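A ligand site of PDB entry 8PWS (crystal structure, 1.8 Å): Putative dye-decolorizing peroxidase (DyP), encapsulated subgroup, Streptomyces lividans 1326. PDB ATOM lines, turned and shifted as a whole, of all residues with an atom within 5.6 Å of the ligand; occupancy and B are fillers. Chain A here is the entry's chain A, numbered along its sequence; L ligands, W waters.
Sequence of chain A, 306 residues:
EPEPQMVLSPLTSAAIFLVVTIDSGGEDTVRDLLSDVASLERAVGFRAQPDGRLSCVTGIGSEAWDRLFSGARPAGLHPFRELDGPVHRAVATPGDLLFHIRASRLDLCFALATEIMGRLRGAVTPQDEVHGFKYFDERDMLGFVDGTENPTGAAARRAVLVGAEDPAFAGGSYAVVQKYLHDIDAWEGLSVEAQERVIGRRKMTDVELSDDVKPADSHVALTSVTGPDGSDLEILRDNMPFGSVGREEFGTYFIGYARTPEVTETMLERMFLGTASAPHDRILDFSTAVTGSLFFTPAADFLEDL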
ATOM      1  N   ASP A 140      17.983  14.703  20.771  1.00  0.00           N
ATOM      2  CA  ASP A 140      19.426  14.724  20.685  1.00  0.00           C
ATOM      3  C   ASP A 140      19.898  15.924  21.519  1.00  0.00           C
ATOM      4  O   ASP A 140      19.178  16.609  22.211  1.00  0.00           O
ATOM      5  CB  ASP A 140      19.900  14.713  19.233  1.00  0.00           C
ATOM      6  CG  ASP A 140      19.400  15.891  18.399  1.00  0.00           C
ATOM      7  OD1 ASP A 140      19.172  16.968  19.000  1.00  0.00           O
ATOM      8  OD2 ASP A 140      19.181  15.680  17.168  1.00  0.00           O
ATOM      9  N   LEU A 142      21.027  18.699  20.635  1.00  0.00           N
ATOM     10  CA  LEU A 142      20.564  20.004  20.215  1.00  0.00           C
ATOM     11  C   LEU A 142      19.139  20.267  20.701  1.00  0.00           C
ATOM     12  O   LEU A 142      18.622  21.338  20.495  1.00  0.00           O
ATOM     13  CB  LEU A 142      20.618  20.087  18.699  1.00  0.00           C
ATOM     14  CG  LEU A 142      21.984  19.870  18.040  1.00  0.00           C
ATOM     15  CD1 LEU A 142      21.877  19.932  16.537  1.00  0.00           C
ATOM     16  CD2 LEU A 142      22.979  20.899  18.545  1.00  0.00           C
ATOM     17  N   PHE A 144      16.337  18.617  19.793  1.00  0.00           N
ATOM     18  CA  PHE A 144      15.306  18.244  18.835  1.00  0.00           C
ATOM     19  C   PHE A 144      15.071  16.739  18.865  1.00  0.00           C
ATOM     20  O   PHE A 144      16.008  15.973  19.100  1.00  0.00           O
ATOM     21  CB  PHE A 144      15.668  18.707  17.440  1.00  0.00           C
ATOM     22  CG  PHE A 144      15.421  20.169  17.211  1.00  0.00           C
ATOM     23  CD1 PHE A 144      16.242  21.128  17.806  1.00  0.00           C
ATOM     24  CD2 PHE A 144      14.428  20.603  16.375  1.00  0.00           C
ATOM     25  CE1 PHE A 144      16.012  22.474  17.586  1.00  0.00           C
ATOM     26  CE2 PHE A 144      14.208  21.959  16.169  1.00  0.00           C
ATOM     27  CZ  PHE A 144      14.992  22.875  16.767  1.00  0.00           C
ATOM     28  N   VAL A 145      13.837  16.327  18.580  1.00  0.00           N
ATOM     29  CA  VAL A 145      13.503  14.915  18.397  1.00  0.00           C
ATOM     30  C   VAL A 145      14.259  14.410  17.180  1.00  0.00           C
ATOM     31  O   VAL A 145      14.341  15.076  16.167  1.00  0.00           O
ATOM     32  CB  VAL A 145      11.971  14.679  18.279  1.00  0.00           C
ATOM     33  CG1 VAL A 145      11.657  13.215  18.109  1.00  0.00           C
ATOM     34  CG2 VAL A 145      11.187  15.257  19.441  1.00  0.00           C
ATOM     35  N   ASP A 146      14.823  13.204  17.317  1.00  0.00           N
ATOM     36  CA  ASP A 146      15.795  12.662  16.376  1.00  0.00           C
ATOM     37  C   ASP A 146      15.327  11.235  16.049  1.00  0.00           C
ATOM     38  O   ASP A 146      15.274  10.402  16.943  1.00  0.00           O
ATOM     39  CB  ASP A 146      17.206  12.775  17.016  1.00  0.00           C
ATOM     40  CG  ASP A 146      18.375  12.487  16.083  1.00  0.00           C
ATOM     41  OD1 ASP A 146      18.211  11.511  15.307  1.00  0.00           O
ATOM     42  OD2 ASP A 146      19.484  13.259  16.130  1.00  0.00           O
ATOM     43  N   GLY A 147      14.950  10.984  14.799  1.00  0.00           N
ATOM     44  CA  GLY A 147      14.428   9.676  14.398  1.00  0.00           C
ATOM     45  C   GLY A 147      13.070   9.678  13.685  1.00  0.00           C
ATOM     46  O   GLY A 147      12.695   8.713  13.048  1.00  0.00           O
ATOM     47  N   THR A 148      12.344  10.794  13.750  1.00  0.00           N
ATOM     48  CA  THR A 148      10.934  10.892  13.407  1.00  0.00           C
ATOM     49  C   THR A 148      10.644  10.383  11.999  1.00  0.00           C
ATOM     50  O   THR A 148       9.695   9.620  11.802  1.00  0.00           O
ATOM     51  CB  THR A 148      10.503  12.336  13.511  1.00  0.00           C
ATOM     52  OG1 THR A 148      10.962  12.866  14.769  1.00  0.00           O
ATOM     53  CG2 THR A 148       8.996  12.477  13.361  1.00  0.00           C
ATOM     54  N   GLU A 149      11.421  10.802  10.996  1.00  0.00           N
ATOM     55  CA  GLU A 149      11.117  10.417   9.629  1.00  0.00           C
ATOM     56  C   GLU A 149      11.862   9.176   9.184  1.00  0.00           C
ATOM     57  O   GLU A 149      11.909   8.878   8.000  1.00  0.00           O
ATOM     58  CB  GLU A 149      11.400  11.598   8.701  1.00  0.00           C
ATOM     59  CG  GLU A 149      10.321  12.673   8.767  1.00  0.00           C
ATOM     60  CD  GLU A 149       8.943  12.187   8.350  1.00  0.00           C
ATOM     61  OE1 GLU A 149       8.801  11.779   7.241  1.00  0.00           O
ATOM     62  OE2 GLU A 149       8.083  12.196   9.178  1.00  0.00           O
ATOM     63  N   ASN A 150      12.437   8.405  10.087  1.00  0.00           N
ATOM     64  CA  ASN A 150      12.998   7.140   9.673  1.00  0.00           C
ATOM     65  C   ASN A 150      11.919   6.304   9.025  1.00  0.00           C
ATOM     66  O   ASN A 150      10.769   6.294   9.499  1.00  0.00           O
ATOM     67  CB  ASN A 150      13.545   6.293  10.806  1.00  0.00           C
ATOM     68  CG  ASN A 150      15.004   6.549  11.075  1.00  0.00           C
ATOM     69  OD1 ASN A 150      15.793   6.816  10.158  1.00  0.00           O
ATOM     70  ND2 ASN A 150      15.360   6.501  12.333  1.00  0.00           N
ATOM     71  N   GLN A 178      29.676   8.703  11.665  1.00  0.00           N
ATOM     72  CA  GLN A 178      30.429   9.908  11.946  1.00  0.00           C
ATOM     73  C   GLN A 178      30.165  10.321  13.393  1.00  0.00           C
ATOM     74  O   GLN A 178      29.023  10.419  13.831  1.00  0.00           O
ATOM     75  CB  GLN A 178      29.926  11.037  11.065  1.00  0.00           C
ATOM     76  CG  GLN A 178      30.183  10.889   9.583  1.00  0.00           C
ATOM     77  CD  GLN A 178      29.652  12.095   8.850  1.00  0.00           C
ATOM     78  OE1 GLN A 178      28.448  12.334   8.849  1.00  0.00           O
ATOM     79  NE2 GLN A 178      30.567  12.894   8.321  1.00  0.00           N
ATOM     80  N   TYR A 180      30.046  13.311  15.833  1.00  0.00           N
ATOM     81  CA  TYR A 180      29.969  14.768  15.797  1.00  0.00           C
ATOM     82  C   TYR A 180      30.051  15.323  17.209  1.00  0.00           C
ATOM     83  O   TYR A 180      29.388  14.812  18.120  1.00  0.00           O
ATOM     84  CB  TYR A 180      28.643  15.261  15.219  1.00  0.00           C
ATOM     85  CG  TYR A 180      28.518  15.170  13.721  1.00  0.00           C
ATOM     86  CD1 TYR A 180      28.951  16.185  12.898  1.00  0.00           C
ATOM     87  CD2 TYR A 180      28.005  14.032  13.130  1.00  0.00           C
ATOM     88  CE1 TYR A 180      28.812  16.088  11.518  1.00  0.00           C
ATOM     89  CE2 TYR A 180      27.935  13.888  11.756  1.00  0.00           C
ATOM     90  CZ  TYR A 180      28.300  14.942  10.947  1.00  0.00           C
ATOM     91  OH  TYR A 180      28.175  14.845   9.572  1.00  0.00           O
ATOM     92  N   HIS A 182      29.235  19.018  19.223  1.00  0.00           N
ATOM     93  CA  HIS A 182      28.461  20.213  19.021  1.00  0.00           C
ATOM     94  C   HIS A 182      29.065  21.360  19.792  1.00  0.00           C
ATOM     95  O   HIS A 182      29.614  21.163  20.875  1.00  0.00           O
ATOM     96  CB  HIS A 182      27.009  19.984  19.459  1.00  0.00           C
ATOM     97  CG  HIS A 182      26.301  18.955  18.651  1.00  0.00           C
ATOM     98  ND1 HIS A 182      26.060  19.154  17.305  1.00  0.00           N
ATOM     99  CD2 HIS A 182      25.824  17.760  19.007  1.00  0.00           C
ATOM    100  CE1 HIS A 182      25.428  18.032  16.873  1.00  0.00           C
ATOM    101  NE2 HIS A 182      25.231  17.188  17.892  1.00  0.00           N
ATOM    102  N   ILE A 199      17.097  23.350  11.604  1.00  0.00           N
ATOM    103  CA  ILE A 199      16.743  21.951  11.512  1.00  0.00           C
ATOM    104  C   ILE A 199      15.689  21.745  10.434  1.00  0.00           C
ATOM    105  O   ILE A 199      15.811  20.816   9.655  1.00  0.00           O
ATOM    106  CB  ILE A 199      16.231  21.461  12.887  1.00  0.00           C
ATOM    107  CG1 ILE A 199      17.296  21.562  13.969  1.00  0.00           C
ATOM    108  CG2 ILE A 199      15.724  20.044  12.784  1.00  0.00           C
ATOM    109  CD1 ILE A 199      18.523  20.757  13.698  1.00  0.00           C
ATOM    110  N   ARG A 201      12.227  21.753  11.495  1.00  0.00           N
ATOM    111  CA  ARG A 201      11.050  21.265  12.202  1.00  0.00           C
ATOM    112  C   ARG A 201      10.851  22.110  13.442  1.00  0.00           C
ATOM    113  O   ARG A 201      11.780  22.759  13.907  1.00  0.00           O
ATOM    114  CB  ARG A 201      11.241  19.808  12.643  1.00  0.00           C
ATOM    115  CG  ARG A 201      11.649  18.853  11.524  1.00  0.00           C
ATOM    116  CD  ARG A 201      11.782  17.421  11.956  1.00  0.00           C
ATOM    117  NE  ARG A 201      10.477  16.810  12.251  1.00  0.00           N
ATOM    118  CZ  ARG A 201       9.681  16.229  11.358  1.00  0.00           C
ATOM    119  NH1 ARG A 201      10.084  15.953  10.127  1.00  0.00           N
ATOM    120  NH2 ARG A 201       8.452  15.894  11.697  1.00  0.00           N
ATOM    121  N   ASP A 206       7.764  18.944  17.158  1.00  0.00           N
ATOM    122  CA  ASP A 206       8.350  18.124  16.112  1.00  0.00           C
ATOM    123  C   ASP A 206       7.500  18.074  14.853  1.00  0.00           C
ATOM    124  O   ASP A 206       7.574  17.140  14.081  1.00  0.00           O
ATOM    125  CB  ASP A 206       8.561  16.680  16.558  1.00  0.00           C
ATOM    126  CG  ASP A 206       9.579  15.902  15.749  1.00  0.00           C
ATOM    127  OD1 ASP A 206      10.436  16.534  15.030  1.00  0.00           O
ATOM    128  OD2 ASP A 206       9.532  14.666  15.868  1.00  0.00           O
ATOM    129  N   GLU A 208       6.982  19.297  11.102  1.00  0.00           N
ATOM    130  CA  GLU A 208       7.803  19.820  10.027  1.00  0.00           C
ATOM    131  C   GLU A 208       7.347  21.227   9.636  1.00  0.00           C
ATOM    132  O   GLU A 208       6.160  21.497   9.628  1.00  0.00           O
ATOM    133  CB  GLU A 208       7.715  18.816   8.869  1.00  0.00           C
ATOM    134  CG  GLU A 208       8.577  19.166   7.687  1.00  0.00           C
ATOM    135  CD  GLU A 208       8.697  18.037   6.676  1.00  0.00           C
ATOM    136  OE1 GLU A 208       8.297  16.901   6.958  1.00  0.00           O
ATOM    137  OE2 GLU A 208       9.346  18.269   5.695  1.00  0.00           O
ATOM    138  N   HIS A 219      18.485  21.406   7.614  1.00  0.00           N
ATOM    139  CA  HIS A 219      18.958  20.029   7.630  1.00  0.00           C
ATOM    140  C   HIS A 219      17.968  19.108   6.917  1.00  0.00           C
ATOM    141  O   HIS A 219      18.377  18.257   6.108  1.00  0.00           O
ATOM    142  CB  HIS A 219      19.243  19.586   9.072  1.00  0.00           C
ATOM    143  CG  HIS A 219      19.730  18.212   9.194  1.00  0.00           C
ATOM    144  ND1 HIS A 219      20.872  17.807   8.551  1.00  0.00           N
ATOM    145  CD2 HIS A 219      19.254  17.130   9.897  1.00  0.00           C
ATOM    146  CE1 HIS A 219      21.105  16.527   8.877  1.00  0.00           C
ATOM    147  NE2 HIS A 219      20.109  16.091   9.679  1.00  0.00           N
ATOM    148  N   VAL A 220      16.675  19.331   7.197  1.00  0.00           N
ATOM    149  CA  VAL A 220      15.639  18.504   6.614  1.00  0.00           C
ATOM    150  C   VAL A 220      15.556  18.732   5.106  1.00  0.00           C
ATOM    151  O   VAL A 220      15.320  17.806   4.353  1.00  0.00           O
ATOM    152  CB  VAL A 220      14.273  18.705   7.316  1.00  0.00           C
ATOM    153  CG1 VAL A 220      13.114  18.230   6.473  1.00  0.00           C
ATOM    154  CG2 VAL A 220      14.291  17.997   8.675  1.00  0.00           C
ATOM    155  N   THR A 223      18.690  16.938   3.385  1.00  0.00           N
ATOM    156  CA  THR A 223      18.779  15.483   3.469  1.00  0.00           C
ATOM    157  C   THR A 223      17.507  14.826   2.913  1.00  0.00           C
ATOM    158  O   THR A 223      17.335  13.629   3.056  1.00  0.00           O
ATOM    159  CB  THR A 223      19.060  15.050   4.920  1.00  0.00           C
ATOM    160  OG1 THR A 223      18.015  15.510   5.802  1.00  0.00           O
ATOM    161  CG2 THR A 223      20.415  15.534   5.398  1.00  0.00           C
ATOM    162  N   SER A 224      16.610  15.601   2.303  1.00  0.00           N
ATOM    163  CA  SER A 224      15.498  15.084   1.521  1.00  0.00           C
ATOM    164  C   SER A 224      15.942  14.966   0.058  1.00  0.00           C
ATOM    165  O   SER A 224      16.354  15.940  -0.541  1.00  0.00           O
ATOM    166  CB  SER A 224      14.280  15.970   1.617  1.00  0.00           C
ATOM    167  OG  SER A 224      13.801  15.958   2.946  1.00  0.00           O
ATOM    168  N   ILE A 235      17.223   6.537   4.204  1.00  0.00           N
ATOM    169  CA  ILE A 235      18.156   5.753   5.001  1.00  0.00           C
ATOM    170  C   ILE A 235      17.542   5.533   6.373  1.00  0.00           C
ATOM    171  O   ILE A 235      16.600   6.185   6.734  1.00  0.00           O
ATOM    172  CB  ILE A 235      19.545   6.431   5.122  1.00  0.00           C
ATOM    173  CG1 ILE A 235      19.507   7.705   5.957  1.00  0.00           C
ATOM    174  CG2 ILE A 235      20.120   6.739   3.764  1.00  0.00           C
ATOM    175  CD1 ILE A 235      20.884   8.238   6.248  1.00  0.00           C
ATOM    176  N   ARG A 237      18.501   5.646  10.354  1.00  0.00           N
ATOM    177  CA  ARG A 237      19.430   6.240  11.276  1.00  0.00           C
ATOM    178  C   ARG A 237      19.129   5.775  12.689  1.00  0.00           C
ATOM    179  O   ARG A 237      17.986   5.537  13.050  1.00  0.00           O
ATOM    180  CB  ARG A 237      19.325   7.778  11.222  1.00  0.00           C
ATOM    181  CG  ARG A 237      19.688   8.381   9.889  1.00  0.00           C
ATOM    182  CD  ARG A 237      19.296   9.840   9.865  1.00  0.00           C
ATOM    183  NE  ARG A 237      17.868   9.985   9.687  1.00  0.00           N
ATOM    184  CZ  ARG A 237      17.054  10.574  10.582  1.00  0.00           C
ATOM    185  NH1 ARG A 237      17.564  11.272  11.578  1.00  0.00           N
ATOM    186  NH2 ARG A 237      15.734  10.477  10.467  1.00  0.00           N
ATOM    187  N   ASN A 239      20.894   7.594  15.548  1.00  0.00           N
ATOM    188  CA  ASN A 239      21.807   8.534  16.183  1.00  0.00           C
ATOM    189  C   ASN A 239      21.683   8.484  17.720  1.00  0.00           C
ATOM    190  O   ASN A 239      20.580   8.359  18.285  1.00  0.00           O
ATOM    191  CB  ASN A 239      21.469   9.962  15.737  1.00  0.00           C
ATOM    192  CG  ASN A 239      21.555  10.149  14.246  1.00  0.00           C
ATOM    193  OD1 ASN A 239      22.133   9.333  13.525  1.00  0.00           O
ATOM    194  ND2 ASN A 239      21.021  11.273  13.774  1.00  0.00           N
ATOM    195  N   THR A 252      26.707  13.940  19.060  1.00  0.00           N
ATOM    196  CA  THR A 252      25.799  13.021  18.390  1.00  0.00           C
ATOM    197  C   THR A 252      26.645  12.009  17.643  1.00  0.00           C
ATOM    198  O   THR A 252      27.490  12.385  16.848  1.00  0.00           O
ATOM    199  CB  THR A 252      24.875  13.747  17.414  1.00  0.00           C
ATOM    200  OG1 THR A 252      24.088  14.724  18.105  1.00  0.00           O
ATOM    201  CG2 THR A 252      23.959  12.814  16.644  1.00  0.00           C
ATOM    202  N   PHE A 254      26.430   9.645  14.807  1.00  0.00           N
ATOM    203  CA  PHE A 254      25.597   9.407  13.645  1.00  0.00           C
ATOM    204  C   PHE A 254      25.874   8.001  13.117  1.00  0.00           C
ATOM    205  O   PHE A 254      27.036   7.658  12.879  1.00  0.00           O
ATOM    206  CB  PHE A 254      25.892  10.396  12.527  1.00  0.00           C
ATOM    207  CG  PHE A 254      25.218  10.055  11.235  1.00  0.00           C
ATOM    208  CD1 PHE A 254      23.887  10.323  11.065  1.00  0.00           C
ATOM    209  CD2 PHE A 254      25.891   9.424  10.239  1.00  0.00           C
ATOM    210  CE1 PHE A 254      23.247  10.006   9.863  1.00  0.00           C
ATOM    211  CE2 PHE A 254      25.239   9.081   9.052  1.00  0.00           C
ATOM    212  CZ  PHE A 254      23.912   9.354   8.888  1.00  0.00           C
ATOM    213  N   THR A 264      23.496   7.544   1.026  1.00  0.00           N
ATOM    214  CA  THR A 264      24.081   8.243   2.146  1.00  0.00           C
ATOM    215  C   THR A 264      25.078   9.283   1.672  1.00  0.00           C
ATOM    216  O   THR A 264      25.137  10.395   2.204  1.00  0.00           O
ATOM    217  CB  THR A 264      24.694   7.248   3.118  1.00  0.00           C
ATOM    218  OG1 THR A 264      23.756   6.247   3.491  1.00  0.00           O
ATOM    219  CG2 THR A 264      25.049   7.880   4.439  1.00  0.00           C
ATOM    220  N   MET A 267      23.493  12.467   0.338  1.00  0.00           N
ATOM    221  CA  MET A 267      23.092  13.327   1.427  1.00  0.00           C
ATOM    222  C   MET A 267      24.306  14.075   2.008  1.00  0.00           C
ATOM    223  O   MET A 267      24.261  15.267   2.284  1.00  0.00           O
ATOM    224  CB  MET A 267      22.432  12.490   2.513  1.00  0.00           C
ATOM    225  CG  MET A 267      21.045  12.034   2.136  1.00  0.00           C
ATOM    226  SD  MET A 267      20.368  10.876   3.351  1.00  0.00           S
ATOM    227  CE  MET A 267      18.814  10.458   2.545  1.00  0.00           C
ATOM    228  N   LEU A 268      25.411  13.367   2.212  1.00  0.00           N
ATOM    229  CA  LEU A 268      26.591  14.011   2.755  1.00  0.00           C
ATOM    230  C   LEU A 268      27.145  15.092   1.822  1.00  0.00           C
ATOM    231  O   LEU A 268      27.607  16.119   2.320  1.00  0.00           O
ATOM    232  CB  LEU A 268      27.671  12.959   3.008  1.00  0.00           C
ATOM    233  CG  LEU A 268      27.455  12.098   4.245  1.00  0.00           C
ATOM    234  CD1 LEU A 268      28.466  10.941   4.249  1.00  0.00           C
ATOM    235  CD2 LEU A 268      27.636  12.951   5.476  1.00  0.00           C
ATOM    236  N   MET A 271      25.061  18.113   2.233  1.00  0.00           N
ATOM    237  CA  MET A 271      25.335  18.766   3.504  1.00  0.00           C
ATOM    238  C   MET A 271      26.649  19.550   3.488  1.00  0.00           C
ATOM    239  O   MET A 271      26.689  20.689   3.967  1.00  0.00           O
ATOM    240  CB  MET A 271      25.378  17.745   4.632  1.00  0.00           C
ATOM    241  CG  MET A 271      24.011  17.187   4.986  1.00  0.00           C
ATOM    242  SD  MET A 271      24.214  15.863   6.249  1.00  0.00           S
ATOM    243  CE  MET A 271      24.829  16.772   7.647  1.00  0.00           C
ATOM    244  N   ILE A 283      23.222  22.844  10.045  1.00  0.00           N
ATOM    245  CA  ILE A 283      23.526  22.099  11.250  1.00  0.00           C
ATOM    246  C   ILE A 283      25.052  21.988  11.464  1.00  0.00           C
ATOM    247  O   ILE A 283      25.528  21.868  12.595  1.00  0.00           O
ATOM    248  CB  ILE A 283      22.848  20.709  11.215  1.00  0.00           C
ATOM    249  CG1 ILE A 283      22.524  20.208  12.615  1.00  0.00           C
ATOM    250  CG2 ILE A 283      23.679  19.681  10.491  1.00  0.00           C
ATOM    251  CD1 ILE A 283      21.675  18.959  12.657  1.00  0.00           C
ATOM    252  N   LEU A 284      25.826  22.039  10.353  1.00  0.00           N
ATOM    253  CA  LEU A 284      27.271  21.923  10.422  1.00  0.00           C
ATOM    254  C   LEU A 284      27.916  23.189  11.008  1.00  0.00           C
ATOM    255  O   LEU A 284      29.055  23.135  11.401  1.00  0.00           O
ATOM    256  CB  LEU A 284      27.824  21.639   9.036  1.00  0.00           C
ATOM    257  CG  LEU A 284      27.386  20.302   8.452  1.00  0.00           C
ATOM    258  CD1 LEU A 284      27.947  20.176   7.062  1.00  0.00           C
ATOM    259  CD2 LEU A 284      27.883  19.151   9.310  1.00  0.00           C
ATOM    260  N   SER A 287      28.229  21.817  14.495  1.00  0.00           N
ATOM    261  CA  SER A 287      28.489  20.377  14.565  1.00  0.00           C
ATOM    262  C   SER A 287      29.767  20.111  13.744  1.00  0.00           C
ATOM    263  O   SER A 287      29.819  20.397  12.534  1.00  0.00           O
ATOM    264  CB  SER A 287      27.355  19.527  14.026  1.00  0.00           C
ATOM    265  OG  SER A 287      26.103  19.928  14.558  1.00  0.00           O
HETATM  266  C1  LIG L   1      16.571  14.249  10.058  1.00  0.00           C
HETATM  267  C2  LIG L   1      19.575  15.539  13.675  1.00  0.00           C
HETATM  268  C3  LIG L   1      23.403  14.285  10.896  1.00  0.00           C
HETATM  269  C4  LIG L   1      20.294  12.523   7.621  1.00  0.00           C
HETATM  270  C5  LIG L   1      17.122  14.724  11.238  1.00  0.00           C
HETATM  271  C6  LIG L   1      16.332  15.431  12.196  1.00  0.00           C
HETATM  272  C7  LIG L   1      17.174  15.758  13.220  1.00  0.00           C
HETATM  273  C8  LIG L   1      18.485  15.361  12.894  1.00  0.00           C
HETATM  274  C9  LIG L   1      16.718  16.451  14.499  1.00  0.00           C
HETATM  275  C10 LIG L   1      14.811  15.689  12.152  1.00  0.00           C
HETATM  276  C11 LIG L   1      13.975  14.511  12.759  1.00  0.00           C
HETATM  277  C12 LIG L   1      14.206  13.193  12.059  1.00  0.00           C
HETATM  278  O1  LIG L   1      15.118  12.421  12.465  1.00  0.00           O
HETATM  279  O2  LIG L   1      13.435  12.915  11.063  1.00  0.00           O
HETATM  280  C13 LIG L   1      20.871  15.295  13.248  1.00  0.00           C
HETATM  281  C14 LIG L   1      22.056  15.573  13.984  1.00  0.00           C
HETATM  282  C15 LIG L   1      23.126  15.231  13.223  1.00  0.00           C
HETATM  283  C16 LIG L   1      22.634  14.728  11.951  1.00  0.00           C
HETATM  284  C17 LIG L   1      22.157  16.142  15.387  1.00  0.00           C
HETATM  285  C18 LIG L   1      24.504  15.555  13.641  1.00  0.00           C
HETATM  286  C19 LIG L   1      25.191  16.332  12.833  1.00  0.00           C
HETATM  287  C20 LIG L   1      22.925  13.703   9.738  1.00  0.00           C
HETATM  288  C21 LIG L   1      23.684  13.158   8.640  1.00  0.00           C
HETATM  289  C22 LIG L   1      22.767  12.688   7.712  1.00  0.00           C
HETATM  290  C23 LIG L   1      21.457  12.943   8.257  1.00  0.00           C
HETATM  291  C24 LIG L   1      25.176  13.143   8.550  1.00  0.00           C
HETATM  292  C25 LIG L   1      22.863  12.007   6.424  1.00  0.00           C
HETATM  293  C26 LIG L   1      24.006  11.727   5.885  1.00  0.00           C
HETATM  294  C27 LIG L   1      19.036  12.828   8.059  1.00  0.00           C
HETATM  295  C28 LIG L   1      17.917  12.453   7.239  1.00  0.00           C
HETATM  296  C29 LIG L   1      16.847  12.947   7.919  1.00  0.00           C
HETATM  297  C30 LIG L   1      17.407  13.679   9.104  1.00  0.00           C
HETATM  298  C31 LIG L   1      17.946  11.624   5.987  1.00  0.00           C
HETATM  299  C32 LIG L   1      15.362  12.795   7.627  1.00  0.00           C
HETATM  300  C33 LIG L   1      14.962  13.921   6.635  1.00  0.00           C
HETATM  301  C34 LIG L   1      13.481  13.876   6.134  1.00  0.00           C
HETATM  302  O3  LIG L   1      13.163  13.286   5.135  1.00  0.00           O
HETATM  303  O4  LIG L   1      12.564  14.468   6.716  1.00  0.00           O
HETATM  304  N1  LIG L   1      18.443  14.737  11.685  1.00  0.00           N
HETATM  305  N2  LIG L   1      21.269  14.793  12.059  1.00  0.00           N
HETATM  306  N3  LIG L   1      21.605  13.521   9.472  1.00  0.00           N
HETATM  307  N4  LIG L   1      18.726  13.562   9.144  1.00  0.00           N
HETATM  308 FE1  LIG L   1      19.950  14.176  10.548  1.00  0.00          FE
HETATM  309  O   HOH W   1      15.345  11.827   3.982  1.00  0.00           O
HETATM  310  O   HOH W   2      12.726  15.117   9.303  1.00  0.00           O
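An iron atom (FE1) of the ligand is bound by a ring nitrogen (NE2) of His 219, at 2.1 Å. O1 of the ligand lies within salt-bridge range of NH1 of Arg 237. An oxygen (O1) of the ligand sits at hydrogen-bond distance from the backbone NH (N) of Thr 148 (3.5 Å). The backbone NH (N) of Glu 149 is in hydrogen-bond range of an oxygen (O2) of the ligand (2.9 Å). N of Gly 147 sits at hydrogen-bond distance from O1 of the ligand (2.7 Å).
The side-chain hydroxyl (OG1) of Thr 252 is in hydrogen-bond range of a ring nitrogen (NE2) of His 182 (2.7 Å). OG of Ser 287 sits at hydrogen-bond distance from O of Ile 283, at 2.8 Å. The guanidinium group (NH1) of Arg 237 is in salt-bridge range of the side-chain carboxylate (OD1) of Asp 146. OD2 of Asp 146 lies close to OD2 of Asp 140 (2.7 Å). OD1 of Asp 146 sits at hydrogen-bond distance from ND2 of Asn 239. O of Ile 199 is in hydrogen-bond range of N of Val 220 (3.0 Å). The guanidinium group of Arg 201 is in salt-bridge range of the side-chain carboxylate of Glu 208, at 3.8 Å. OG1 of Thr 148 lies within hydrogen-bond range of OD2 of Asp 206 (2.5 Å).
OD2 of Asp 140 touches C17 of the ligand, 3.5 Å away. Leu 142 touches the ligand (CD1 to C17, 3.97 Å). CB of Phe 144 touches C9 of the ligand, 3.9 Å away. Val 145 touches the ligand (O to C9, 3.2 Å). Asp 146 touches the ligand (OD2 to C2, 3.4 Å). Gln 178 touches the ligand. Tyr 180 touches the ligand. Arg 201 touches the ligand (CD to C10, 3.5 Å). Val 220 touches the ligand (CG1 to O4, 3.8 Å). Thr 223 touches the ligand (OG1 to C28, 3.4 Å). OG of Ser 224 touches O3 of the ligand, 3.5 Å away. Asn 239 touches the ligand. OG1 of Thr 252 touches C17 of the ligand, at 3.6 Å. CE1 of Phe 254 touches C21 of the ligand, at 3.4 Å. SD of Met 267 touches C31 of the ligand, at 3.7 Å. Leu 268 touches the ligand (CG to C26, 3.8 Å). Met 271 touches the ligand. Ile 283 touches the ligand (CD1 to C14, 3.7 Å). Within 4 Å of the ligand: Asp 140, Leu 142, Phe 144, Val 145, Asp 146, Gly 147, Thr 148, Glu 149, Gln 178, Tyr 180, Arg 201, His 219, Val 220, Thr 223, Ser 224, Arg 237, Asn 239, Thr 252, Phe 254, Met 267, Leu 268, Met 271 and Ile 283. Along chain A the residues within 4 Å of the ligand span positions 140 to 283.
Water W2 bridges O4 of the ligand and NH1 of Arg 201. Water W1 bridges the backbone carbonyl oxygen of Thr 223 (2.8 Å) and an oxygen (O3) of the ligand (2.9 Å).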
